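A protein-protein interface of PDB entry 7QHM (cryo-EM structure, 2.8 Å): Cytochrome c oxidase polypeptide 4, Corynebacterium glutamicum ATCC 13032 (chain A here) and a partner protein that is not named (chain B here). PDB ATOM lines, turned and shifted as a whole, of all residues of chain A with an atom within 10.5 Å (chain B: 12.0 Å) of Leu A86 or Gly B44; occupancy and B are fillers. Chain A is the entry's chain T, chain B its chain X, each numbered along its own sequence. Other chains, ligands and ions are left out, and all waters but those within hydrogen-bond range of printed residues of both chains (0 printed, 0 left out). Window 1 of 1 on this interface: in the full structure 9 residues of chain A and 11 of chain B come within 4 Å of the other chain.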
ATOM      1  N   LEU A  70     -14.423   1.349  12.425  1.00  0.00           N
ATOM      2  CA  LEU A  70     -14.635   0.180  13.255  1.00  0.00           C
ATOM      3  C   LEU A  70     -13.332  -0.242  13.917  1.00  0.00           C
ATOM      4  O   LEU A  70     -12.249   0.085  13.431  1.00  0.00           O
ATOM      5  CB  LEU A  70     -15.190  -0.966  12.418  1.00  0.00           C
ATOM      6  CG  LEU A  70     -16.449  -0.644  11.618  1.00  0.00           C
ATOM      7  CD1 LEU A  70     -16.854  -1.842  10.781  1.00  0.00           C
ATOM      8  CD2 LEU A  70     -17.585  -0.216  12.525  1.00  0.00           C
ATOM      9  N   PRO A  71     -13.403  -0.966  15.036  1.00  0.00           N
ATOM     10  CA  PRO A  71     -12.157  -1.406  15.669  1.00  0.00           C
ATOM     11  C   PRO A  71     -11.366  -2.384  14.823  1.00  0.00           C
ATOM     12  O   PRO A  71     -10.132  -2.365  14.879  1.00  0.00           O
ATOM     13  CB  PRO A  71     -12.637  -2.035  16.981  1.00  0.00           C
ATOM     14  CG  PRO A  71     -14.054  -2.340  16.766  1.00  0.00           C
ATOM     15  CD  PRO A  71     -14.575  -1.316  15.853  1.00  0.00           C
ATOM     16  N   GLU A  72     -12.023  -3.229  14.032  1.00  0.00           N
ATOM     17  CA  GLU A  72     -11.287  -4.145  13.167  1.00  0.00           C
ATOM     18  C   GLU A  72     -10.676  -3.459  11.954  1.00  0.00           C
ATOM     19  O   GLU A  72      -9.919  -4.106  11.226  1.00  0.00           O
ATOM     20  CB  GLU A  72     -12.182  -5.287  12.694  1.00  0.00           C
ATOM     21  CG  GLU A  72     -13.438  -4.869  11.990  1.00  0.00           C
ATOM     22  CD  GLU A  72     -14.641  -4.977  12.877  1.00  0.00           C
ATOM     23  OE1 GLU A  72     -14.580  -4.507  14.034  1.00  0.00           O
ATOM     24  OE2 GLU A  72     -15.655  -5.544  12.421  1.00  0.00           O
ATOM     25  N   VAL A  79      -9.048  -4.846  22.659  1.00  0.00           N
ATOM     26  CA  VAL A  79      -9.902  -6.016  22.495  1.00  0.00           C
ATOM     27  C   VAL A  79     -11.305  -5.765  23.029  1.00  0.00           C
ATOM     28  O   VAL A  79     -12.249  -6.444  22.617  1.00  0.00           O
ATOM     29  CB  VAL A  79      -9.256  -7.238  23.178  1.00  0.00           C
ATOM     30  CG1 VAL A  79     -10.110  -8.479  23.004  1.00  0.00           C
ATOM     31  CG2 VAL A  79      -7.862  -7.493  22.621  1.00  0.00           C
ATOM     32  N   ASP A  81     -13.222  -3.189  22.527  1.00  0.00           N
ATOM     33  CA  ASP A  81     -14.027  -2.274  21.726  1.00  0.00           C
ATOM     34  C   ASP A  81     -15.191  -2.978  21.034  1.00  0.00           C
ATOM     35  O   ASP A  81     -16.207  -2.337  20.742  1.00  0.00           O
ATOM     36  CB  ASP A  81     -13.144  -1.582  20.688  1.00  0.00           C
ATOM     37  CG  ASP A  81     -13.772  -0.313  20.132  1.00  0.00           C
ATOM     38  OD1 ASP A  81     -14.939  -0.016  20.459  1.00  0.00           O
ATOM     39  OD2 ASP A  81     -13.090   0.398  19.367  1.00  0.00           O
ATOM     40  N   LYS A  82     -15.071  -4.276  20.760  1.00  0.00           N
ATOM     41  CA  LYS A  82     -16.152  -5.064  20.188  1.00  0.00           C
ATOM     42  C   LYS A  82     -16.963  -5.799  21.244  1.00  0.00           C
ATOM     43  O   LYS A  82     -17.758  -6.678  20.900  1.00  0.00           O
ATOM     44  CB  LYS A  82     -15.597  -6.060  19.163  1.00  0.00           C
ATOM     45  CG  LYS A  82     -15.254  -5.411  17.844  1.00  0.00           C
ATOM     46  CD  LYS A  82     -14.924  -6.425  16.759  1.00  0.00           C
ATOM     47  CE  LYS A  82     -16.168  -7.076  16.175  1.00  0.00           C
ATOM     48  NZ  LYS A  82     -15.887  -7.697  14.850  1.00  0.00           N
ATOM     49  N   ALA A  83     -16.795  -5.458  22.516  1.00  0.00           N
ATOM     50  CA  ALA A  83     -17.590  -6.092  23.553  1.00  0.00           C
ATOM     51  C   ALA A  83     -19.051  -5.688  23.407  1.00  0.00           C
ATOM     52  O   ALA A  83     -19.368  -4.519  23.174  1.00  0.00           O
ATOM     53  CB  ALA A  83     -17.066  -5.708  24.934  1.00  0.00           C
ATOM     54  N   GLY A  84     -19.938  -6.668  23.549  1.00  0.00           N
ATOM     55  CA  GLY A  84     -21.358  -6.519  23.348  1.00  0.00           C
ATOM     56  C   GLY A  84     -21.867  -7.623  22.456  1.00  0.00           C
ATOM     57  O   GLY A  84     -21.229  -8.668  22.306  1.00  0.00           O
ATOM     58  N   THR A  85     -23.024  -7.395  21.849  1.00  0.00           N
ATOM     59  CA  THR A  85     -23.556  -8.358  20.901  1.00  0.00           C
ATOM     60  C   THR A  85     -22.787  -8.293  19.590  1.00  0.00           C
ATOM     61  O   THR A  85     -22.441  -7.214  19.104  1.00  0.00           O
ATOM     62  CB  THR A  85     -25.036  -8.099  20.648  1.00  0.00           C
ATOM     63  OG1 THR A  85     -25.747  -8.156  21.890  1.00  0.00           O
ATOM     64  CG2 THR A  85     -25.613  -9.135  19.694  1.00  0.00           C
ATOM     65  N   LEU A  86     -22.518  -9.465  19.026  1.00  0.00           N
ATOM     66  CA  LEU A  86     -21.888  -9.601  17.724  1.00  0.00           C
ATOM     67  C   LEU A  86     -22.889  -9.924  16.629  1.00  0.00           C
ATOM     68  O   LEU A  86     -22.701  -9.498  15.487  1.00  0.00           O
ATOM     69  CB  LEU A  86     -20.822 -10.696  17.777  1.00  0.00           C
ATOM     70  CG  LEU A  86     -19.820 -10.757  16.630  1.00  0.00           C
ATOM     71  CD1 LEU A  86     -18.799  -9.644  16.723  1.00  0.00           C
ATOM     72  CD2 LEU A  86     -19.129 -12.092  16.614  1.00  0.00           C
ATOM     73  N   GLY A  87     -23.935 -10.662  16.951  1.00  0.00           N
ATOM     74  CA  GLY A  87     -25.007 -10.932  16.014  1.00  0.00           C
ATOM     75  C   GLY A  87     -25.600 -12.300  16.254  1.00  0.00           C
ATOM     76  O   GLY A  87     -25.122 -13.082  17.068  1.00  0.00           O
ATOM     77  N   PHE A  88     -26.658 -12.582  15.508  1.00  0.00           N
ATOM     78  CA  PHE A  88     -27.355 -13.853  15.586  1.00  0.00           C
ATOM     79  C   PHE A  88     -26.772 -14.839  14.589  1.00  0.00           C
ATOM     80  O   PHE A  88     -26.480 -14.484  13.446  1.00  0.00           O
ATOM     81  CB  PHE A  88     -28.842 -13.648  15.320  1.00  0.00           C
ATOM     82  CG  PHE A  88     -29.615 -14.917  15.190  1.00  0.00           C
ATOM     83  CD1 PHE A  88     -29.928 -15.667  16.296  1.00  0.00           C
ATOM     84  CD2 PHE A  88     -30.038 -15.357  13.962  1.00  0.00           C
ATOM     85  CE1 PHE A  88     -30.636 -16.827  16.173  1.00  0.00           C
ATOM     86  CE2 PHE A  88     -30.750 -16.519  13.845  1.00  0.00           C
ATOM     87  CZ  PHE A  88     -31.045 -17.252  14.950  1.00  0.00           C
ATOM     88  N   PHE A  89     -26.592 -16.079  15.036  1.00  0.00           N
ATOM     89  CA  PHE A  89     -26.069 -17.156  14.212  1.00  0.00           C
ATOM     90  C   PHE A  89     -26.907 -18.396  14.458  1.00  0.00           C
ATOM     91  O   PHE A  89     -27.279 -18.687  15.594  1.00  0.00           O
ATOM     92  CB  PHE A  89     -24.603 -17.452  14.532  1.00  0.00           C
ATOM     93  CG  PHE A  89     -23.670 -16.313  14.244  1.00  0.00           C
ATOM     94  CD1 PHE A  89     -23.542 -15.264  15.125  1.00  0.00           C
ATOM     95  CD2 PHE A  89     -22.911 -16.302  13.091  1.00  0.00           C
ATOM     96  CE1 PHE A  89     -22.688 -14.220  14.858  1.00  0.00           C
ATOM     97  CE2 PHE A  89     -22.047 -15.266  12.825  1.00  0.00           C
ATOM     98  CZ  PHE A  89     -21.938 -14.222  13.712  1.00  0.00           C
ATOM     99  N   SER A  90     -27.213 -19.116  13.399  1.00  0.00           N
ATOM    100  CA  SER A  90     -27.987 -20.339  13.513  1.00  0.00           C
ATOM    101  C   SER A  90     -27.204 -21.381  14.311  1.00  0.00           C
ATOM    102  O   SER A  90     -26.067 -21.696  13.933  1.00  0.00           O
ATOM    103  CB  SER A  90     -28.308 -20.876  12.125  1.00  0.00           C
ATOM    104  OG  SER A  90     -28.837 -22.186  12.190  1.00  0.00           O
ATOM    105  N   VAL B  34     -33.127   2.347  12.096  1.00  0.00           N
ATOM    106  CA  VAL B  34     -32.598   1.213  12.841  1.00  0.00           C
ATOM    107  C   VAL B  34     -31.728   0.368  11.931  1.00  0.00           C
ATOM    108  O   VAL B  34     -30.636  -0.066  12.311  1.00  0.00           O
ATOM    109  CB  VAL B  34     -33.748   0.389  13.447  1.00  0.00           C
ATOM    110  CG1 VAL B  34     -33.200  -0.795  14.214  1.00  0.00           C
ATOM    111  CG2 VAL B  34     -34.603   1.252  14.358  1.00  0.00           C
ATOM    112  N   VAL B  35     -32.197   0.132  10.712  1.00  0.00           N
ATOM    113  CA  VAL B  35     -31.477  -0.654   9.726  1.00  0.00           C
ATOM    114  C   VAL B  35     -31.805  -0.084   8.357  1.00  0.00           C
ATOM    115  O   VAL B  35     -32.919   0.385   8.119  1.00  0.00           O
ATOM    116  CB  VAL B  35     -31.863  -2.149   9.836  1.00  0.00           C
ATOM    117  CG1 VAL B  35     -33.364  -2.361   9.606  1.00  0.00           C
ATOM    118  CG2 VAL B  35     -31.052  -2.987   8.883  1.00  0.00           C
ATOM    119  N   THR B  36     -30.830  -0.111   7.453  1.00  0.00           N
ATOM    120  CA  THR B  36     -31.122   0.130   6.052  1.00  0.00           C
ATOM    121  C   THR B  36     -30.232  -0.768   5.217  1.00  0.00           C
ATOM    122  O   THR B  36     -29.313  -1.418   5.725  1.00  0.00           O
ATOM    123  CB  THR B  36     -30.939   1.594   5.647  1.00  0.00           C
ATOM    124  OG1 THR B  36     -31.289   1.746   4.269  1.00  0.00           O
ATOM    125  CG2 THR B  36     -29.512   2.049   5.850  1.00  0.00           C
ATOM    126  N   GLU B  37     -30.484  -0.739   3.908  1.00  0.00           N
ATOM    127  CA  GLU B  37     -29.976  -1.779   3.024  1.00  0.00           C
ATOM    128  C   GLU B  37     -28.463  -1.834   3.040  1.00  0.00           C
ATOM    129  O   GLU B  37     -27.880  -2.914   2.919  1.00  0.00           O
ATOM    130  CB  GLU B  37     -30.443  -1.552   1.589  1.00  0.00           C
ATOM    131  CG  GLU B  37     -31.919  -1.307   1.356  1.00  0.00           C
ATOM    132  CD  GLU B  37     -32.140  -0.313   0.243  1.00  0.00           C
ATOM    133  OE1 GLU B  37     -31.674   0.837   0.376  1.00  0.00           O
ATOM    134  OE2 GLU B  37     -32.761  -0.681  -0.773  1.00  0.00           O
ATOM    135  N   LEU B  38     -27.810  -0.690   3.203  1.00  0.00           N
ATOM    136  CA  LEU B  38     -26.357  -0.668   3.196  1.00  0.00           C
ATOM    137  C   LEU B  38     -25.777  -1.022   4.554  1.00  0.00           C
ATOM    138  O   LEU B  38     -24.747  -1.698   4.620  1.00  0.00           O
ATOM    139  CB  LEU B  38     -25.858   0.707   2.764  1.00  0.00           C
ATOM    140  CG  LEU B  38     -26.084   1.067   1.302  1.00  0.00           C
ATOM    141  CD1 LEU B  38     -26.013   2.556   1.124  1.00  0.00           C
ATOM    142  CD2 LEU B  38     -25.062   0.388   0.423  1.00  0.00           C
ATOM    143  N   ILE B  39     -26.410  -0.585   5.647  1.00  0.00           N
ATOM    144  CA  ILE B  39     -25.768  -0.597   6.958  1.00  0.00           C
ATOM    145  C   ILE B  39     -26.735  -1.068   8.035  1.00  0.00           C
ATOM    146  O   ILE B  39     -27.961  -0.969   7.912  1.00  0.00           O
ATOM    147  CB  ILE B  39     -25.189   0.786   7.352  1.00  0.00           C
ATOM    148  CG1 ILE B  39     -26.288   1.830   7.495  1.00  0.00           C
ATOM    149  CG2 ILE B  39     -24.168   1.269   6.335  1.00  0.00           C
ATOM    150  CD1 ILE B  39     -26.742   2.076   8.918  1.00  0.00           C
ATOM    151  N   SER B  40     -26.147  -1.574   9.113  1.00  0.00           N
ATOM    152  CA  SER B  40     -26.877  -1.989  10.297  1.00  0.00           C
ATOM    153  C   SER B  40     -26.064  -1.586  11.520  1.00  0.00           C
ATOM    154  O   SER B  40     -24.954  -1.058  11.407  1.00  0.00           O
ATOM    155  CB  SER B  40     -27.169  -3.494  10.261  1.00  0.00           C
ATOM    156  OG  SER B  40     -25.989  -4.251  10.075  1.00  0.00           O
ATOM    157  N   LYS B  41     -26.634  -1.808  12.702  1.00  0.00           N
ATOM    158  CA  LYS B  41     -25.965  -1.520  13.963  1.00  0.00           C
ATOM    159  C   LYS B  41     -25.338  -2.763  14.577  1.00  0.00           C
ATOM    160  O   LYS B  41     -25.052  -2.777  15.776  1.00  0.00           O
ATOM    161  CB  LYS B  41     -26.944  -0.887  14.954  1.00  0.00           C
ATOM    162  CG  LYS B  41     -27.848   0.216  14.388  1.00  0.00           C
ATOM    163  CD  LYS B  41     -27.090   1.411  13.835  1.00  0.00           C
ATOM    164  CE  LYS B  41     -26.406   2.196  14.924  1.00  0.00           C
ATOM    165  NZ  LYS B  41     -26.039   3.564  14.478  1.00  0.00           N
ATOM    166  N   VAL B  42     -25.097  -3.798  13.777  1.00  0.00           N
ATOM    167  CA  VAL B  42     -24.606  -5.075  14.272  1.00  0.00           C
ATOM    168  C   VAL B  42     -23.737  -5.688  13.187  1.00  0.00           C
ATOM    169  O   VAL B  42     -23.895  -5.386  12.004  1.00  0.00           O
ATOM    170  CB  VAL B  42     -25.779  -6.000  14.677  1.00  0.00           C
ATOM    171  CG1 VAL B  42     -26.713  -6.273  13.498  1.00  0.00           C
ATOM    172  CG2 VAL B  42     -25.274  -7.290  15.280  1.00  0.00           C
ATOM    173  N   ALA B  43     -22.801  -6.537  13.600  1.00  0.00           N
ATOM    174  CA  ALA B  43     -21.824  -7.116  12.688  1.00  0.00           C
ATOM    175  C   ALA B  43     -22.333  -8.369  11.993  1.00  0.00           C
ATOM    176  O   ALA B  43     -21.945  -8.633  10.851  1.00  0.00           O
ATOM    177  CB  ALA B  43     -20.537  -7.441  13.446  1.00  0.00           C
ATOM    178  N   GLY B  44     -23.184  -9.140  12.649  1.00  0.00           N
ATOM    179  CA  GLY B  44     -23.809 -10.308  12.074  1.00  0.00           C
ATOM    180  C   GLY B  44     -25.227 -10.035  11.628  1.00  0.00           C
ATOM    181  O   GLY B  44     -25.564  -8.936  11.178  1.00  0.00           O
ATOM    182  N   ALA B  45     -26.071 -11.047  11.759  1.00  0.00           N
ATOM    183  CA  ALA B  45     -27.489 -10.910  11.480  1.00  0.00           C
ATOM    184  C   ALA B  45     -28.209 -10.419  12.723  1.00  0.00           C
ATOM    185  O   ALA B  45     -27.852 -10.782  13.844  1.00  0.00           O
ATOM    186  CB  ALA B  45     -28.079 -12.241  11.024  1.00  0.00           C
ATOM    187  N   SER B  46     -29.214  -9.581  12.525  1.00  0.00           N
ATOM    188  CA  SER B  46     -30.060  -9.183  13.635  1.00  0.00           C
ATOM    189  C   SER B  46     -30.855 -10.383  14.131  1.00  0.00           C
ATOM    190  O   SER B  46     -31.205 -11.282  13.363  1.00  0.00           O
ATOM    191  CB  SER B  46     -31.004  -8.063  13.216  1.00  0.00           C
ATOM    192  OG  SER B  46     -30.343  -6.819  13.254  1.00  0.00           O
ATOM    193  N   SER B  47     -31.140 -10.392  15.415  1.00  0.00           N
ATOM    194  CA  SER B  47     -31.738 -11.584  15.989  1.00  0.00           C
ATOM    195  C   SER B  47     -33.244 -11.598  15.734  1.00  0.00           C
ATOM    196  O   SER B  47     -33.882 -10.546  15.771  1.00  0.00           O
ATOM    197  CB  SER B  47     -31.467 -11.654  17.485  1.00  0.00           C
ATOM    198  OG  SER B  47     -32.059 -10.569  18.160  1.00  0.00           O
ATOM    199  N   PRO B  48     -33.848 -12.770  15.498  1.00  0.00           N
ATOM    200  CA  PRO B  48     -35.311 -12.818  15.385  1.00  0.00           C
ATOM    201  C   PRO B  48     -36.038 -12.391  16.644  1.00  0.00           C
ATOM    202  O   PRO B  48     -37.229 -12.076  16.571  1.00  0.00           O
ATOM    203  CB  PRO B  48     -35.589 -14.294  15.075  1.00  0.00           C
ATOM    204  CG  PRO B  48     -34.333 -14.848  14.635  1.00  0.00           C
ATOM    205  CD  PRO B  48     -33.272 -14.112  15.325  1.00  0.00           C
ATOM    206  N   TRP B  49     -35.362 -12.370  17.792  1.00  0.00           N
ATOM    207  CA  TRP B  49     -35.993 -12.129  19.080  1.00  0.00           C
ATOM    208  C   TRP B  49     -35.904 -10.671  19.498  1.00  0.00           C
ATOM    209  O   TRP B  49     -36.050 -10.364  20.683  1.00  0.00           O
ATOM    210  CB  TRP B  49     -35.364 -13.005  20.164  1.00  0.00           C
ATOM    211  CG  TRP B  49     -34.654 -14.214  19.686  1.00  0.00           C
ATOM    212  CD1 TRP B  49     -33.333 -14.476  19.815  1.00  0.00           C
ATOM    213  CD2 TRP B  49     -35.220 -15.326  18.997  1.00  0.00           C
ATOM    214  NE1 TRP B  49     -33.032 -15.683  19.254  1.00  0.00           N
ATOM    215  CE2 TRP B  49     -34.177 -16.228  18.742  1.00  0.00           C
ATOM    216  CE3 TRP B  49     -36.507 -15.647  18.568  1.00  0.00           C
ATOM    217  CZ2 TRP B  49     -34.381 -17.427  18.079  1.00  0.00           C
ATOM    218  CZ3 TRP B  49     -36.706 -16.826  17.915  1.00  0.00           C
ATOM    219  CH2 TRP B  49     -35.650 -17.707  17.673  1.00  0.00           C
ATOM    220  N   GLY B  50     -35.654  -9.768  18.558  1.00  0.00           N
ATOM    221  CA  GLY B  50     -35.513  -8.371  18.887  1.00  0.00           C
ATOM    222  C   GLY B  50     -34.202  -8.093  19.580  1.00  0.00           C
ATOM    223  O   GLY B  50     -33.902  -8.695  20.611  1.00  0.00           O
ATOM    224  N   ASP B  51     -33.403  -7.187  19.020  1.00  0.00           N
ATOM    225  CA  ASP B  51     -32.123  -6.858  19.633  1.00  0.00           C
ATOM    226  C   ASP B  51     -32.286  -5.998  20.878  1.00  0.00           C
ATOM    227  O   ASP B  51     -31.352  -5.907  21.680  1.00  0.00           O
ATOM    228  CB  ASP B  51     -31.226  -6.154  18.617  1.00  0.00           C
ATOM    229  CG  ASP B  51     -30.878  -7.042  17.439  1.00  0.00           C
ATOM    230  OD1 ASP B  51     -30.662  -8.250  17.648  1.00  0.00           O
ATOM    231  OD2 ASP B  51     -30.819  -6.532  16.303  1.00  0.00           O
ATOM    232  N   ASP B  52     -33.446  -5.371  21.060  1.00  0.00           N
ATOM    233  CA  ASP B  52     -33.689  -4.621  22.282  1.00  0.00           C
ATOM    234  C   ASP B  52     -33.846  -5.537  23.483  1.00  0.00           C
ATOM    235  O   ASP B  52     -33.683  -5.083  24.620  1.00  0.00           O
ATOM    236  CB  ASP B  52     -34.934  -3.749  22.121  1.00  0.00           C
ATOM    237  CG  ASP B  52     -35.213  -2.895  23.346  1.00  0.00           C
ATOM    238  OD1 ASP B  52     -34.326  -2.109  23.742  1.00  0.00           O
ATOM    239  OD2 ASP B  52     -36.318  -3.010  23.914  1.00  0.00           O
ATOM    240  N   LYS B  53     -34.149  -6.809  23.258  1.00  0.00           N
ATOM    241  CA  LYS B  53     -34.266  -7.760  24.348  1.00  0.00           C
ATOM    242  C   LYS B  53     -32.894  -8.064  24.928  1.00  0.00           C
ATOM    243  O   LYS B  53     -31.877  -8.011  24.232  1.00  0.00           O
ATOM    244  CB  LYS B  53     -34.920  -9.045  23.850  1.00  0.00           C
ATOM    245  CG  LYS B  53     -35.428  -9.983  24.932  1.00  0.00           C
ATOM    246  CD  LYS B  53     -36.586  -9.417  25.764  1.00  0.00           C
ATOM    247  CE  LYS B  53     -37.808  -9.065  24.919  1.00  0.00           C
ATOM    248  NZ  LYS B  53     -38.987  -8.731  25.760  1.00  0.00           N
ATOM    249  N   GLU B  54     -32.873  -8.366  26.222  1.00  0.00           N
ATOM    250  CA  GLU B  54     -31.681  -8.843  26.909  1.00  0.00           C
ATOM    251  C   GLU B  54     -32.007 -10.202  27.496  1.00  0.00           C
ATOM    252  O   GLU B  54     -32.958 -10.330  28.273  1.00  0.00           O
ATOM    253  CB  GLU B  54     -31.236  -7.873  28.004  1.00  0.00           C
ATOM    254  CG  GLU B  54     -29.878  -8.202  28.631  1.00  0.00           C
ATOM    255  CD  GLU B  54     -28.721  -8.045  27.659  1.00  0.00           C
ATOM    256  OE1 GLU B  54     -28.908  -7.404  26.604  1.00  0.00           O
ATOM    257  OE2 GLU B  54     -27.625  -8.566  27.952  1.00  0.00           O
ATOM    258  N   PHE B  55     -31.238 -11.207  27.102  1.00  0.00           N
ATOM    259  CA  PHE B  55     -31.339 -12.563  27.601  1.00  0.00           C
ATOM    260  C   PHE B  55     -30.175 -12.857  28.535  1.00  0.00           C
ATOM    261  O   PHE B  55     -29.144 -12.182  28.479  1.00  0.00           O
ATOM    262  CB  PHE B  55     -31.332 -13.566  26.440  1.00  0.00           C
ATOM    263  CG  PHE B  55     -32.631 -13.658  25.712  1.00  0.00           C
ATOM    264  CD1 PHE B  55     -33.640 -14.477  26.176  1.00  0.00           C
ATOM    265  CD2 PHE B  55     -32.844 -12.938  24.551  1.00  0.00           C
ATOM    266  CE1 PHE B  55     -34.840 -14.556  25.508  1.00  0.00           C
ATOM    267  CE2 PHE B  55     -34.041 -13.020  23.879  1.00  0.00           C
ATOM    268  CZ  PHE B  55     -35.038 -13.826  24.358  1.00  0.00           C
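The backbone carbonyl oxygen (O) of Leu A86 lies within hydrogen-bond range of the backbone NH (N) of Gly B44 (2.9 Å).
The backbone carbonyl oxygen (O) of Ala B45 sits at hydrogen-bond distance from the backbone NH (N) of Phe A88.
The side-chain hydroxyl (OG) of Ser B46 is in hydrogen-bond range of the side-chain carboxylate (OD2) of Asp B51, at 3.1 Å.
The side-chain hydroxyl (OG) of Ser B47 lies within hydrogen-bond range of the side-chain carboxylate (OD1) of Asp B51, at 2.8 Å.
The side-chain hydroxyl (OG) of Ser B40 sits at hydrogen-bond distance from the backbone carbonyl oxygen (O) of Val B42 (3.1 Å).
Val B42 touches Leu A86.
N of Ala B43 touches O of Leu A86 (3.5 Å).
Val B42 touches Gly A87.
Gly A87 touches Ala B45.
Phe A88 touches Ser B46.
Phe A88 touches Ser B47.
Phe A88 touches Pro B48 (CD2 to CD, 3.7 Å).
Of the printed residues of chain B, Leu A86 touches Val B42 (3.4 Å), Ala B43 (3.5 Å) and Gly B44 (2.9 Å).
Gly B44 touches just one residue of chain A: Leu A86.
No residue of chain B comes within 4 Å of Lys A82.
No residue of chain B comes within 4 Å of Gly A84.
No residue of chain B comes within 4 Å of Thr A85.
Gly A87 touches two residues of chain B.
Ala B43 touches one residue of chain A.
Ala B45 touches two residues of chain A.
Ser B46 touches just one residue of chain A: Phe A88.
Printed residues of chain B within 4 Å of Phe A88: Ala B45 (2.7 Å), Ser B46 (3.9 Å), Ser B47 (3.6 Å) and Pro B48 (3.7 Å).
Of the printed residues of chain A, Pro B48 touches Phe A88 (3.7 Å).
Of the printed residues of chain A, Ser B47 touches Phe A88 (3.6 Å).
Val B35 touches none of the printed residues of chain A.
Ile B39 touches none of the printed residues of chain A.
The nearest residue of chain B that does not touch Leu A86 is Ala B45 (5.3 Å).
The nearest printed residue of chain A that does not touch Pro B48 is Phe A89 (7.0 Å).
Of the 14 printed residues of chain A, 3 touch a printed residue of chain B.
Printed residues of chain A that touch a printed residue of chain B: Leu A86, Gly A87 and Phe A88.
Hydrophobic or aromatic side chains of chain A that line the printed part of chain B: Phe A88.
Of the 22 printed residues of chain B, 7 touch a printed residue of chain A.
Hydrophobic or aromatic side chains of chain B within 4 Å of the printed part of chain A: Val B42, Ala B43, Ala B45 and Pro B48.
Along chain B the printed residues that touch a printed residue of chain A span positions 42 to 48.
Among the printed residues, 9 pairs touch across the chains.
Among the printed residues, no Asp or Glu carboxylate lies within 4 Å of a Lys or Arg side-chain nitrogen of the other chain.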
